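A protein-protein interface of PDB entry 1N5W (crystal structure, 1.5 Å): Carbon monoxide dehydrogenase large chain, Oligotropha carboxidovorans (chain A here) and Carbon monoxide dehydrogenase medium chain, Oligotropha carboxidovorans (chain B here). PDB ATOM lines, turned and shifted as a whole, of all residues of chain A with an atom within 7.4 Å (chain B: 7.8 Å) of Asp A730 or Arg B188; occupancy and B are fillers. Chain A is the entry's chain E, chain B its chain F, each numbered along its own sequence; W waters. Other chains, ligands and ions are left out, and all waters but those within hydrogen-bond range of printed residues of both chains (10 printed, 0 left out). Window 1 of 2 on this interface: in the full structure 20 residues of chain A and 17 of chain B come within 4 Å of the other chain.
N of Ile B190 lies within hydrogen-bond range of OE2 of Glu A738 (2.8 Å).
The side-chain carboxylate of Asp A730 is in salt-bridge range of the guanidinium group of Arg B188 (2.9 Å).
The backbone carbonyl oxygen of Leu A733 sits at hydrogen-bond distance from the side-chain amino group of Lys B189.
The guanidinium group (NH2) of Arg B188 is in hydrogen-bond range of the backbone carbonyl oxygen (O) of Met A729.
Asp A730 touches just one residue of chain B: Arg B188.
Arg B188 touches just these residues of chain A: Met A729 (3.2 Å), Asp A730 (2.9 Å) and Phe A732 (3.6 Å).
Printed residues of chain B within 4 Å of Trp A796: Gly B260, Arg B261 and Gly B262.
Of the printed residues of chain A, Gly B260 touches Trp A796 (3.9 Å).
Ala B194 touches none of the printed residues of chain A.
Gln A713 touches none of the printed residues of chain B.
The nearest residue of chain A that does not touch Arg B188 is Glu A738 (4.7 Å).
The nearest printed residue of chain B that does not touch Glu A738 is Arg B188 (4.7 Å).
Water W10 lies within hydrogen-bond range of O of Phe A731, NZ of Lys B189 and O of Phe A728.
Water W8 lies within hydrogen-bond range of OD1 of Asp B192, O of Met A729 and NH2 of Arg B261.
Water W7 lies within hydrogen-bond range of O of Gly B260 (2.7 Å), OE2 of Glu A714 (2.8 Å) and NE1 of Trp A796 (3.0 Å).
Water W5 bridges the guanidinium group of Arg A716 (3.0 Å) and the backbone carbonyl oxygen of Asp B259 (3.0 Å).
Water W4 bridges NH1 of Arg A716 (3.1 Å) and O of Asp B259 (3.3 Å).
Water W1 lies within hydrogen-bond range of the backbone carbonyl oxygen of Gly B191 (3.2 Å) and the side-chain sulfur of Met A729 (3.2 Å).
Arg B188 touches Phe A732 (O to CE1, 3.6 Å).
CA of Lys B189 touches OE2 of Glu A738, at 3.3 Å.
NE1 of Trp A796 touches O of Gly B260, at 3.9 Å.
Arg B261 touches Trp A796.
CG of Trp A796 touches CA of Gly B262 (3.6 Å).
The backbone carbonyl oxygen (O) of Tyr B193 sits at hydrogen-bond distance from the guanidinium group (NE) of Arg B261.
OG of Ser A727 sits at hydrogen-bond distance from N of Met A729.
O of Phe A732 is in hydrogen-bond range of NE2 of Gln A713 (2.8 Å).
OD2 of Asp B259 is in salt-bridge range of NH1 of Arg B261 (3.2 Å).
NH1 of Arg B188 sits close to O of Gly B260 (3.5 Å).
The side-chain carboxylate (OD1) of Asp B192 is in salt-bridge range of the guanidinium group (NH2) of Arg B261, at 2.9 Å.
Of the 15 printed residues of chain B, 6 touch a printed residue of chain A.
Printed residues of chain B that touch a printed residue of chain A: Arg B188, Lys B189, Ile B190, Gly B260, Arg B261 and Gly B262.
Hydrophobic or aromatic side chains of chain A that line the printed part of chain B: Phe A732 and Trp A796.
Along chain A the printed residues that touch a printed residue of chain B span positions 729 to 796.
Among the printed residues, 9 pairs touch across the chains.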
ATOM      1  N   GLY A 712     -25.617  23.681 -24.882  1.00  0.00           N
ATOM      2  CA  GLY A 712     -25.204  22.609 -23.946  1.00  0.00           C
ATOM      3  C   GLY A 712     -26.252  21.690 -23.376  1.00  0.00           C
ATOM      4  O   GLY A 712     -25.928  20.569 -22.971  1.00  0.00           O
ATOM      5  N   GLN A 713     -27.490  22.152 -23.151  1.00  0.00           N
ATOM      6  CA  GLN A 713     -28.442  21.368 -22.344  1.00  0.00           C
ATOM      7  C   GLN A 713     -28.942  20.151 -23.075  1.00  0.00           C
ATOM      8  O   GLN A 713     -29.187  20.215 -24.301  1.00  0.00           O
ATOM      9  CB  GLN A 713     -29.646  22.230 -21.961  1.00  0.00           C
ATOM     10  CG  GLN A 713     -29.385  23.074 -20.763  1.00  0.00           C
ATOM     11  CD  GLN A 713     -30.599  23.890 -20.256  1.00  0.00           C
ATOM     12  OE1 GLN A 713     -31.603  24.035 -20.941  1.00  0.00           O
ATOM     13  NE2 GLN A 713     -30.435  24.574 -19.157  1.00  0.00           N
ATOM     14  N   GLU A 714     -29.206  19.055 -22.349  1.00  0.00           N
ATOM     15  CA  GLU A 714     -29.760  17.838 -22.936  1.00  0.00           C
ATOM     16  C   GLU A 714     -30.185  16.911 -21.807  1.00  0.00           C
ATOM     17  O   GLU A 714     -29.559  16.916 -20.720  1.00  0.00           O
ATOM     18  CB  GLU A 714     -28.741  17.103 -23.863  1.00  0.00           C
ATOM     19  CG  GLU A 714     -27.513  16.662 -23.122  1.00  0.00           C
ATOM     20  CD  GLU A 714     -26.373  16.133 -24.006  1.00  0.00           C
ATOM     21  OE1 GLU A 714     -26.619  15.852 -25.232  1.00  0.00           O
ATOM     22  OE2 GLU A 714     -25.263  15.898 -23.457  1.00  0.00           O
ATOM     23  N   ARG A 716     -30.685  12.705 -22.059  1.00  0.00           N
ATOM     24  CA  ARG A 716     -30.490  11.601 -22.990  1.00  0.00           C
ATOM     25  C   ARG A 716     -30.895  10.259 -22.401  1.00  0.00           C
ATOM     26  O   ARG A 716     -31.074  10.140 -21.192  1.00  0.00           O
ATOM     27  CB  ARG A 716     -29.036  11.515 -23.492  1.00  0.00           C
ATOM     28  CG  ARG A 716     -28.679  12.735 -24.329  1.00  0.00           C
ATOM     29  CD  ARG A 716     -27.333  12.604 -24.955  1.00  0.00           C
ATOM     30  NE  ARG A 716     -26.350  12.608 -23.896  1.00  0.00           N
ATOM     31  CZ  ARG A 716     -25.093  12.269 -24.051  1.00  0.00           C
ATOM     32  NH1 ARG A 716     -24.335  12.208 -22.968  1.00  0.00           N
ATOM     33  NH2 ARG A 716     -24.647  11.819 -25.242  1.00  0.00           N
ATOM     34  N   LEU A 724     -29.689   9.748 -18.841  1.00  0.00           N
ATOM     35  CA  LEU A 724     -28.327  10.262 -18.736  1.00  0.00           C
ATOM     36  C   LEU A 724     -28.354  11.771 -18.641  1.00  0.00           C
ATOM     37  O   LEU A 724     -29.085  12.464 -19.376  1.00  0.00           O
ATOM     38  CB  LEU A 724     -27.517   9.907 -19.976  1.00  0.00           C
ATOM     39  CG  LEU A 724     -27.473   8.430 -20.338  1.00  0.00           C
ATOM     40  CD1 LEU A 724     -26.588   8.181 -21.550  1.00  0.00           C
ATOM     41  CD2 LEU A 724     -26.944   7.686 -19.157  1.00  0.00           C
ATOM     42  N   GLY A 725     -27.516  12.278 -17.735  1.00  0.00           N
ATOM     43  CA  GLY A 725     -27.318  13.703 -17.628  1.00  0.00           C
ATOM     44  C   GLY A 725     -28.372  14.445 -16.824  1.00  0.00           C
ATOM     45  O   GLY A 725     -28.343  15.678 -16.832  1.00  0.00           O
ATOM     46  N   ALA A 726     -29.221  13.717 -16.106  1.00  0.00           N
ATOM     47  CA  ALA A 726     -30.329  14.331 -15.401  1.00  0.00           C
ATOM     48  C   ALA A 726     -29.976  14.750 -13.979  1.00  0.00           C
ATOM     49  O   ALA A 726     -30.609  14.314 -12.987  1.00  0.00           O
ATOM     50  CB  ALA A 726     -31.568  13.470 -15.407  1.00  0.00           C
ATOM     51  N   SER A 727     -28.953  15.586 -13.855  1.00  0.00           N
ATOM     52  CA  SER A 727     -28.593  16.217 -12.581  1.00  0.00           C
ATOM     53  C   SER A 727     -27.768  17.428 -12.929  1.00  0.00           C
ATOM     54  O   SER A 727     -27.258  17.521 -14.044  1.00  0.00           O
ATOM     55  CB  SER A 727     -27.755  15.302 -11.718  1.00  0.00           C
ATOM     56  OG  SER A 727     -26.394  15.269 -12.072  1.00  0.00           O
ATOM     57  N   PHE A 728     -27.525  18.302 -11.971  1.00  0.00           N
ATOM     58  CA  PHE A 728     -26.688  19.468 -12.210  1.00  0.00           C
ATOM     59  C   PHE A 728     -25.198  19.119 -12.374  1.00  0.00           C
ATOM     60  O   PHE A 728     -24.388  19.992 -12.632  1.00  0.00           O
ATOM     61  CB  PHE A 728     -26.948  20.562 -11.164  1.00  0.00           C
ATOM     62  CG  PHE A 728     -28.330  21.211 -11.256  1.00  0.00           C
ATOM     63  CD1 PHE A 728     -29.153  21.058 -12.347  1.00  0.00           C
ATOM     64  CD2 PHE A 728     -28.746  22.048 -10.239  1.00  0.00           C
ATOM     65  CE1 PHE A 728     -30.383  21.712 -12.421  1.00  0.00           C
ATOM     66  CE2 PHE A 728     -29.970  22.731 -10.305  1.00  0.00           C
ATOM     67  CZ  PHE A 728     -30.813  22.536 -11.381  1.00  0.00           C
ATOM     68  N   MET A 729     -24.799  17.854 -12.169  1.00  0.00           N
ATOM     69  CA  MET A 729     -23.442  17.441 -12.544  1.00  0.00           C
ATOM     70  C   MET A 729     -23.207  17.586 -14.044  1.00  0.00           C
ATOM     71  O   MET A 729     -22.069  17.817 -14.464  1.00  0.00           O
ATOM     72  CB  MET A 729     -23.142  15.982 -12.177  1.00  0.00           C
ATOM     73  CG  MET A 729     -21.666  15.706 -12.031  1.00  0.00           C
ATOM     74  SD  MET A 729     -21.007  16.400 -10.475  1.00  0.00           S
ATOM     75  CE  MET A 729     -22.255  16.014  -9.484  1.00  0.00           C
ATOM     76  N   ASP A 730     -24.267  17.434 -14.866  1.00  0.00           N
ATOM     77  CA  ASP A 730     -24.118  17.438 -16.305  1.00  0.00           C
ATOM     78  C   ASP A 730     -25.058  18.395 -17.052  1.00  0.00           C
ATOM     79  O   ASP A 730     -24.711  18.871 -18.121  1.00  0.00           O
ATOM     80  CB  ASP A 730     -24.374  16.048 -16.830  1.00  0.00           C
ATOM     81  CG  ASP A 730     -23.296  15.062 -16.400  1.00  0.00           C
ATOM     82  OD1 ASP A 730     -22.131  15.156 -16.874  1.00  0.00           O
ATOM     83  OD2 ASP A 730     -23.581  14.247 -15.476  1.00  0.00           O
ATOM     84  N   PHE A 731     -26.219  18.702 -16.458  1.00  0.00           N
ATOM     85  CA  PHE A 731     -27.272  19.460 -17.120  1.00  0.00           C
ATOM     86  C   PHE A 731     -26.834  20.922 -17.149  1.00  0.00           C
ATOM     87  O   PHE A 731     -26.641  21.532 -16.108  1.00  0.00           O
ATOM     88  CB  PHE A 731     -28.623  19.311 -16.378  1.00  0.00           C
ATOM     89  CG  PHE A 731     -29.792  19.958 -17.080  1.00  0.00           C
ATOM     90  CD1 PHE A 731     -30.343  19.378 -18.215  1.00  0.00           C
ATOM     91  CD2 PHE A 731     -30.288  21.192 -16.676  1.00  0.00           C
ATOM     92  CE1 PHE A 731     -31.375  19.981 -18.938  1.00  0.00           C
ATOM     93  CE2 PHE A 731     -31.378  21.766 -17.361  1.00  0.00           C
ATOM     94  CZ  PHE A 731     -31.913  21.173 -18.486  1.00  0.00           C
ATOM     95  N   PHE A 732     -26.617  21.498 -18.320  1.00  0.00           N
ATOM     96  CA  PHE A 732     -25.919  22.783 -18.463  1.00  0.00           C
ATOM     97  C   PHE A 732     -26.820  23.963 -18.080  1.00  0.00           C
ATOM     98  O   PHE A 732     -27.646  24.440 -18.863  1.00  0.00           O
ATOM     99  CB  PHE A 732     -25.486  22.968 -19.929  1.00  0.00           C
ATOM    100  CG  PHE A 732     -24.732  24.263 -20.188  1.00  0.00           C
ATOM    101  CD1 PHE A 732     -23.476  24.503 -19.614  1.00  0.00           C
ATOM    102  CD2 PHE A 732     -25.233  25.209 -21.051  1.00  0.00           C
ATOM    103  CE1 PHE A 732     -22.806  25.646 -19.897  1.00  0.00           C
ATOM    104  CE2 PHE A 732     -24.569  26.387 -21.331  1.00  0.00           C
ATOM    105  CZ  PHE A 732     -23.334  26.599 -20.712  1.00  0.00           C
ATOM    106  N   LEU A 733     -26.739  24.433 -16.851  1.00  0.00           N
ATOM    107  CA  LEU A 733     -27.341  25.694 -16.458  1.00  0.00           C
ATOM    108  C   LEU A 733     -26.242  26.694 -16.316  1.00  0.00           C
ATOM    109  O   LEU A 733     -25.342  26.502 -15.473  1.00  0.00           O
ATOM    110  CB  LEU A 733     -28.074  25.531 -15.151  1.00  0.00           C
ATOM    111  CG  LEU A 733     -29.512  24.989 -15.187  1.00  0.00           C
ATOM    112  CD1 LEU A 733     -30.134  25.006 -13.780  1.00  0.00           C
ATOM    113  CD2 LEU A 733     -30.390  25.725 -16.217  1.00  0.00           C
ATOM    114  N   GLU A 738     -20.678  32.203 -17.617  1.00  0.00           N
ATOM    115  CA  GLU A 738     -20.947  31.751 -18.995  1.00  0.00           C
ATOM    116  C   GLU A 738     -22.000  32.589 -19.706  1.00  0.00           C
ATOM    117  O   GLU A 738     -22.053  32.572 -20.933  1.00  0.00           O
ATOM    118  CB  GLU A 738     -21.383  30.289 -19.040  1.00  0.00           C
ATOM    119  CG  GLU A 738     -20.335  29.304 -18.613  1.00  0.00           C
ATOM    120  CD  GLU A 738     -20.203  29.133 -17.106  1.00  0.00           C
ATOM    121  OE1 GLU A 738     -21.237  29.346 -16.384  1.00  0.00           O
ATOM    122  OE2 GLU A 738     -19.100  28.834 -16.623  1.00  0.00           O
ATOM    123  N   ASP A 794     -22.154  22.111 -28.011  1.00  0.00           N
ATOM    124  CA  ASP A 794     -21.110  22.123 -26.990  1.00  0.00           C
ATOM    125  C   ASP A 794     -19.740  21.802 -27.585  1.00  0.00           C
ATOM    126  O   ASP A 794     -19.610  21.482 -28.767  1.00  0.00           O
ATOM    127  CB  ASP A 794     -21.441  21.256 -25.768  1.00  0.00           C
ATOM    128  CG  ASP A 794     -21.631  19.791 -26.082  1.00  0.00           C
ATOM    129  OD1 ASP A 794     -21.427  19.414 -27.285  1.00  0.00           O
ATOM    130  OD2 ASP A 794     -21.968  19.008 -25.139  1.00  0.00           O
ATOM    131  N   ALA A 795     -18.722  21.821 -26.748  1.00  0.00           N
ATOM    132  CA  ALA A 795     -17.351  21.761 -27.320  1.00  0.00           C
ATOM    133  C   ALA A 795     -17.004  20.451 -27.988  1.00  0.00           C
ATOM    134  O   ALA A 795     -16.428  20.417 -29.062  1.00  0.00           O
ATOM    135  CB  ALA A 795     -16.322  22.171 -26.310  1.00  0.00           C
ATOM    136  N   TRP A 796     -17.400  19.334 -27.386  1.00  0.00           N
ATOM    137  CA  TRP A 796     -17.027  18.062 -27.970  1.00  0.00           C
ATOM    138  C   TRP A 796     -17.731  17.904 -29.328  1.00  0.00           C
ATOM    139  O   TRP A 796     -17.144  17.341 -30.261  1.00  0.00           O
ATOM    140  CB  TRP A 796     -17.260  16.867 -27.045  1.00  0.00           C
ATOM    141  CG  TRP A 796     -18.624  16.317 -26.866  1.00  0.00           C
ATOM    142  CD1 TRP A 796     -19.430  16.567 -25.785  1.00  0.00           C
ATOM    143  CD2 TRP A 796     -19.328  15.358 -27.653  1.00  0.00           C
ATOM    144  NE1 TRP A 796     -20.601  15.863 -25.856  1.00  0.00           N
ATOM    145  CE2 TRP A 796     -20.562  15.108 -27.011  1.00  0.00           C
ATOM    146  CE3 TRP A 796     -19.052  14.696 -28.879  1.00  0.00           C
ATOM    147  CZ2 TRP A 796     -21.514  14.219 -27.535  1.00  0.00           C
ATOM    148  CZ3 TRP A 796     -19.982  13.804 -29.381  1.00  0.00           C
ATOM    149  CH2 TRP A 796     -21.211  13.571 -28.700  1.00  0.00           C
ATOM    150  N   LYS B 185      -7.094  24.480 -17.878  1.00  0.00           N
ATOM    151  CA  LYS B 185      -8.228  23.578 -17.712  1.00  0.00           C
ATOM    152  C   LYS B 185      -9.312  23.822 -18.742  1.00  0.00           C
ATOM    153  O   LYS B 185      -9.716  24.987 -18.949  1.00  0.00           O
ATOM    154  CB  LYS B 185      -8.799  23.762 -16.304  1.00  0.00           C
ATOM    155  CG  LYS B 185      -9.928  22.876 -15.903  1.00  0.00           C
ATOM    156  CD  LYS B 185     -10.247  22.932 -14.396  1.00  0.00           C
ATOM    157  CE  LYS B 185     -11.509  22.165 -13.995  1.00  0.00           C
ATOM    158  NZ  LYS B 185     -11.737  22.186 -12.552  1.00  0.00           N
ATOM    159  N   LEU B 186      -9.813  22.746 -19.307  1.00  0.00           N
ATOM    160  CA  LEU B 186     -10.957  22.804 -20.227  1.00  0.00           C
ATOM    161  C   LEU B 186     -12.108  22.187 -19.442  1.00  0.00           C
ATOM    162  O   LEU B 186     -12.014  21.063 -18.987  1.00  0.00           O
ATOM    163  CB  LEU B 186     -10.671  22.039 -21.517  1.00  0.00           C
ATOM    164  CG  LEU B 186     -11.779  21.978 -22.557  1.00  0.00           C
ATOM    165  CD1 LEU B 186     -12.120  23.386 -23.161  1.00  0.00           C
ATOM    166  CD2 LEU B 186     -11.470  21.039 -23.687  1.00  0.00           C
ATOM    167  N   LYS B 187     -13.224  22.907 -19.345  1.00  0.00           N
ATOM    168  CA  LYS B 187     -14.389  22.449 -18.597  1.00  0.00           C
ATOM    169  C   LYS B 187     -15.687  22.952 -19.243  1.00  0.00           C
ATOM    170  O   LYS B 187     -15.663  23.932 -20.005  1.00  0.00           O
ATOM    171  CB  LYS B 187     -14.298  22.888 -17.137  1.00  0.00           C
ATOM    172  CG  LYS B 187     -14.388  24.410 -16.978  1.00  0.00           C
ATOM    173  CD  LYS B 187     -13.840  24.943 -15.679  1.00  0.00           C
ATOM    174  CE  LYS B 187     -14.120  26.431 -15.529  1.00  0.00           C
ATOM    175  NZ  LYS B 187     -13.404  27.250 -16.494  1.00  0.00           N
ATOM    176  N   ARG B 188     -16.834  22.365 -18.867  1.00  0.00           N
ATOM    177  CA  ARG B 188     -18.093  22.767 -19.477  1.00  0.00           C
ATOM    178  C   ARG B 188     -18.652  24.065 -18.911  1.00  0.00           C
ATOM    179  O   ARG B 188     -19.332  24.815 -19.609  1.00  0.00           O
ATOM    180  CB  ARG B 188     -19.162  21.663 -19.340  1.00  0.00           C
ATOM    181  CG  ARG B 188     -18.903  20.445 -20.186  1.00  0.00           C
ATOM    182  CD  ARG B 188     -19.788  19.261 -19.892  1.00  0.00           C
ATOM    183  NE  ARG B 188     -19.594  18.745 -18.549  1.00  0.00           N
ATOM    184  CZ  ARG B 188     -20.255  17.731 -18.048  1.00  0.00           C
ATOM    185  NH1 ARG B 188     -21.204  17.112 -18.779  1.00  0.00           N
ATOM    186  NH2 ARG B 188     -20.010  17.329 -16.806  1.00  0.00           N
ATOM    187  N   LYS B 189     -18.325  24.375 -17.670  1.00  0.00           N
ATOM    188  CA  LYS B 189     -18.771  25.548 -16.966  1.00  0.00           C
ATOM    189  C   LYS B 189     -18.016  25.662 -15.650  1.00  0.00           C
ATOM    190  O   LYS B 189     -17.389  24.691 -15.214  1.00  0.00           O
ATOM    191  CB  LYS B 189     -20.282  25.586 -16.707  1.00  0.00           C
ATOM    192  CG  LYS B 189     -20.829  24.272 -16.085  1.00  0.00           C
ATOM    193  CD  LYS B 189     -22.304  24.307 -15.724  1.00  0.00           C
ATOM    194  CE  LYS B 189     -22.487  24.704 -14.356  1.00  0.00           C
ATOM    195  NZ  LYS B 189     -23.958  24.705 -13.892  1.00  0.00           N
ATOM    196  N   ILE B 190     -18.098  26.808 -15.023  1.00  0.00           N
ATOM    197  CA  ILE B 190     -17.723  26.953 -13.625  1.00  0.00           C
ATOM    198  C   ILE B 190     -18.221  25.785 -12.775  1.00  0.00           C
ATOM    199  O   ILE B 190     -19.388  25.380 -12.829  1.00  0.00           O
ATOM    200  CB  ILE B 190     -18.364  28.272 -13.026  1.00  0.00           C
ATOM    201  CG1 ILE B 190     -17.739  29.482 -13.649  1.00  0.00           C
ATOM    202  CG2 ILE B 190     -18.240  28.245 -11.495  1.00  0.00           C
ATOM    203  CD1 ILE B 190     -16.267  29.641 -13.318  1.00  0.00           C
ATOM    204  N   GLY B 191     -17.314  25.243 -11.984  1.00  0.00           N
ATOM    205  CA  GLY B 191     -17.612  24.210 -11.039  1.00  0.00           C
ATOM    206  C   GLY B 191     -17.496  22.802 -11.560  1.00  0.00           C
ATOM    207  O   GLY B 191     -17.758  21.824 -10.853  1.00  0.00           O
ATOM    208  N   ASP B 192     -17.278  22.653 -12.846  1.00  0.00           N
ATOM    209  CA  ASP B 192     -17.141  21.303 -13.400  1.00  0.00           C
ATOM    210  C   ASP B 192     -15.712  20.742 -13.276  1.00  0.00           C
ATOM    211  O   ASP B 192     -14.688  21.456 -13.450  1.00  0.00           O
ATOM    212  CB  ASP B 192     -17.599  21.345 -14.846  1.00  0.00           C
ATOM    213  CG  ASP B 192     -17.869  20.022 -15.502  1.00  0.00           C
ATOM    214  OD1 ASP B 192     -18.103  18.993 -14.857  1.00  0.00           O
ATOM    215  OD2 ASP B 192     -17.819  20.016 -16.757  1.00  0.00           O
ATOM    216  N   TYR B 193     -15.673  19.413 -13.174  1.00  0.00           N
ATOM    217  CA  TYR B 193     -14.424  18.695 -13.323  1.00  0.00           C
ATOM    218  C   TYR B 193     -13.922  18.779 -14.771  1.00  0.00           C
ATOM    219  O   TYR B 193     -14.719  18.827 -15.704  1.00  0.00           O
ATOM    220  CB  TYR B 193     -14.546  17.253 -12.842  1.00  0.00           C
ATOM    221  CG  TYR B 193     -15.037  17.111 -11.414  1.00  0.00           C
ATOM    222  CD1 TYR B 193     -16.375  16.946 -11.152  1.00  0.00           C
ATOM    223  CD2 TYR B 193     -14.188  17.327 -10.319  1.00  0.00           C
ATOM    224  CE1 TYR B 193     -16.844  16.895  -9.862  1.00  0.00           C
ATOM    225  CE2 TYR B 193     -14.628  17.230  -9.043  1.00  0.00           C
ATOM    226  CZ  TYR B 193     -15.953  16.970  -8.802  1.00  0.00           C
ATOM    227  OH  TYR B 193     -16.378  16.921  -7.497  1.00  0.00           O
ATOM    228  N   ALA B 194     -12.598  18.696 -14.984  1.00  0.00           N
ATOM    229  CA  ALA B 194     -12.018  18.955 -16.297  1.00  0.00           C
ATOM    230  C   ALA B 194     -12.432  17.937 -17.330  1.00  0.00           C
ATOM    231  O   ALA B 194     -12.352  16.721 -17.132  1.00  0.00           O
ATOM    232  CB  ALA B 194     -10.507  19.001 -16.224  1.00  0.00           C
ATOM    233  N   THR B 195     -12.739  18.414 -18.532  1.00  0.00           N
ATOM    234  CA  THR B 195     -12.691  17.608 -19.742  1.00  0.00           C
ATOM    235  C   THR B 195     -11.264  17.079 -19.907  1.00  0.00           C
ATOM    236  O   THR B 195     -11.039  15.866 -20.168  1.00  0.00           O
ATOM    237  CB  THR B 195     -13.152  18.468 -20.925  1.00  0.00           C
ATOM    238  OG1 THR B 195     -14.511  18.879 -20.659  1.00  0.00           O
ATOM    239  CG2 THR B 195     -13.133  17.686 -22.241  1.00  0.00           C
ATOM    240  N   ASP B 259     -17.822  10.387 -21.316  1.00  0.00           N
ATOM    241  CA  ASP B 259     -18.962  10.784 -20.513  1.00  0.00           C
ATOM    242  C   ASP B 259     -19.586  12.043 -21.079  1.00  0.00           C
ATOM    243  O   ASP B 259     -19.458  12.321 -22.297  1.00  0.00           O
ATOM    244  CB  ASP B 259     -18.614  10.820 -18.996  1.00  0.00           C
ATOM    245  CG  ASP B 259     -17.580  11.869 -18.620  1.00  0.00           C
ATOM    246  OD1 ASP B 259     -17.468  12.935 -19.252  1.00  0.00           O
ATOM    247  OD2 ASP B 259     -16.761  11.631 -17.668  1.00  0.00           O
ATOM    248  N   GLY B 260     -20.343  12.778 -20.266  1.00  0.00           N
ATOM    249  CA  GLY B 260     -20.948  14.028 -20.719  1.00  0.00           C
ATOM    250  C   GLY B 260     -19.991  15.088 -21.214  1.00  0.00           C
ATOM    251  O   GLY B 260     -20.388  15.978 -21.960  1.00  0.00           O
ATOM    252  N   ARG B 261     -18.736  14.962 -20.864  1.00  0.00           N
ATOM    253  CA  ARG B 261     -17.672  15.847 -21.322  1.00  0.00           C
ATOM    254  C   ARG B 261     -17.140  15.535 -22.718  1.00  0.00           C
ATOM    255  O   ARG B 261     -16.327  16.291 -23.300  1.00  0.00           O
ATOM    256  CB  ARG B 261     -16.545  15.866 -20.286  1.00  0.00           C
ATOM    257  CG  ARG B 261     -16.936  16.460 -18.926  1.00  0.00           C
ATOM    258  CD  ARG B 261     -15.858  16.149 -17.866  1.00  0.00           C
ATOM    259  NE  ARG B 261     -16.403  16.492 -16.558  1.00  0.00           N
ATOM    260  CZ  ARG B 261     -17.216  15.699 -15.902  1.00  0.00           C
ATOM    261  NH1 ARG B 261     -17.481  14.507 -16.344  1.00  0.00           N
ATOM    262  NH2 ARG B 261     -17.760  16.077 -14.777  1.00  0.00           N
ATOM    263  N   GLY B 262     -17.607  14.404 -23.241  1.00  0.00           N
ATOM    264  CA  GLY B 262     -17.230  13.935 -24.568  1.00  0.00           C
ATOM    265  C   GLY B 262     -16.527  12.591 -24.560  1.00  0.00           C
ATOM    266  O   GLY B 262     -16.344  11.999 -23.506  1.00  0.00           O
HETATM  267  O   HOH W   1     -19.457  19.216 -10.318  1.00  0.00           O
HETATM  268  O   HOH W   2     -21.081  12.783 -17.461  1.00  0.00           O
HETATM  269  O   HOH W   3     -20.123  18.579 -23.077  1.00  0.00           O
HETATM  270  O   HOH W   4     -21.937  10.224 -22.716  1.00  0.00           O
HETATM  271  O   HOH W   5     -21.693  12.717 -24.206  1.00  0.00           O
HETATM  272  O   HOH W   6     -22.962  17.837 -20.925  1.00  0.00           O
HETATM  273  O   HOH W   7     -22.506  15.406 -23.569  1.00  0.00           O
HETATM  274  O   HOH W   8     -19.722  17.999 -12.929  1.00  0.00           O
HETATM  275  O   HOH W   9     -19.291  17.722  -7.754  1.00  0.00           O
HETATM  276  O   HOH W  10     -25.378  22.309 -13.883  1.00  0.00           O
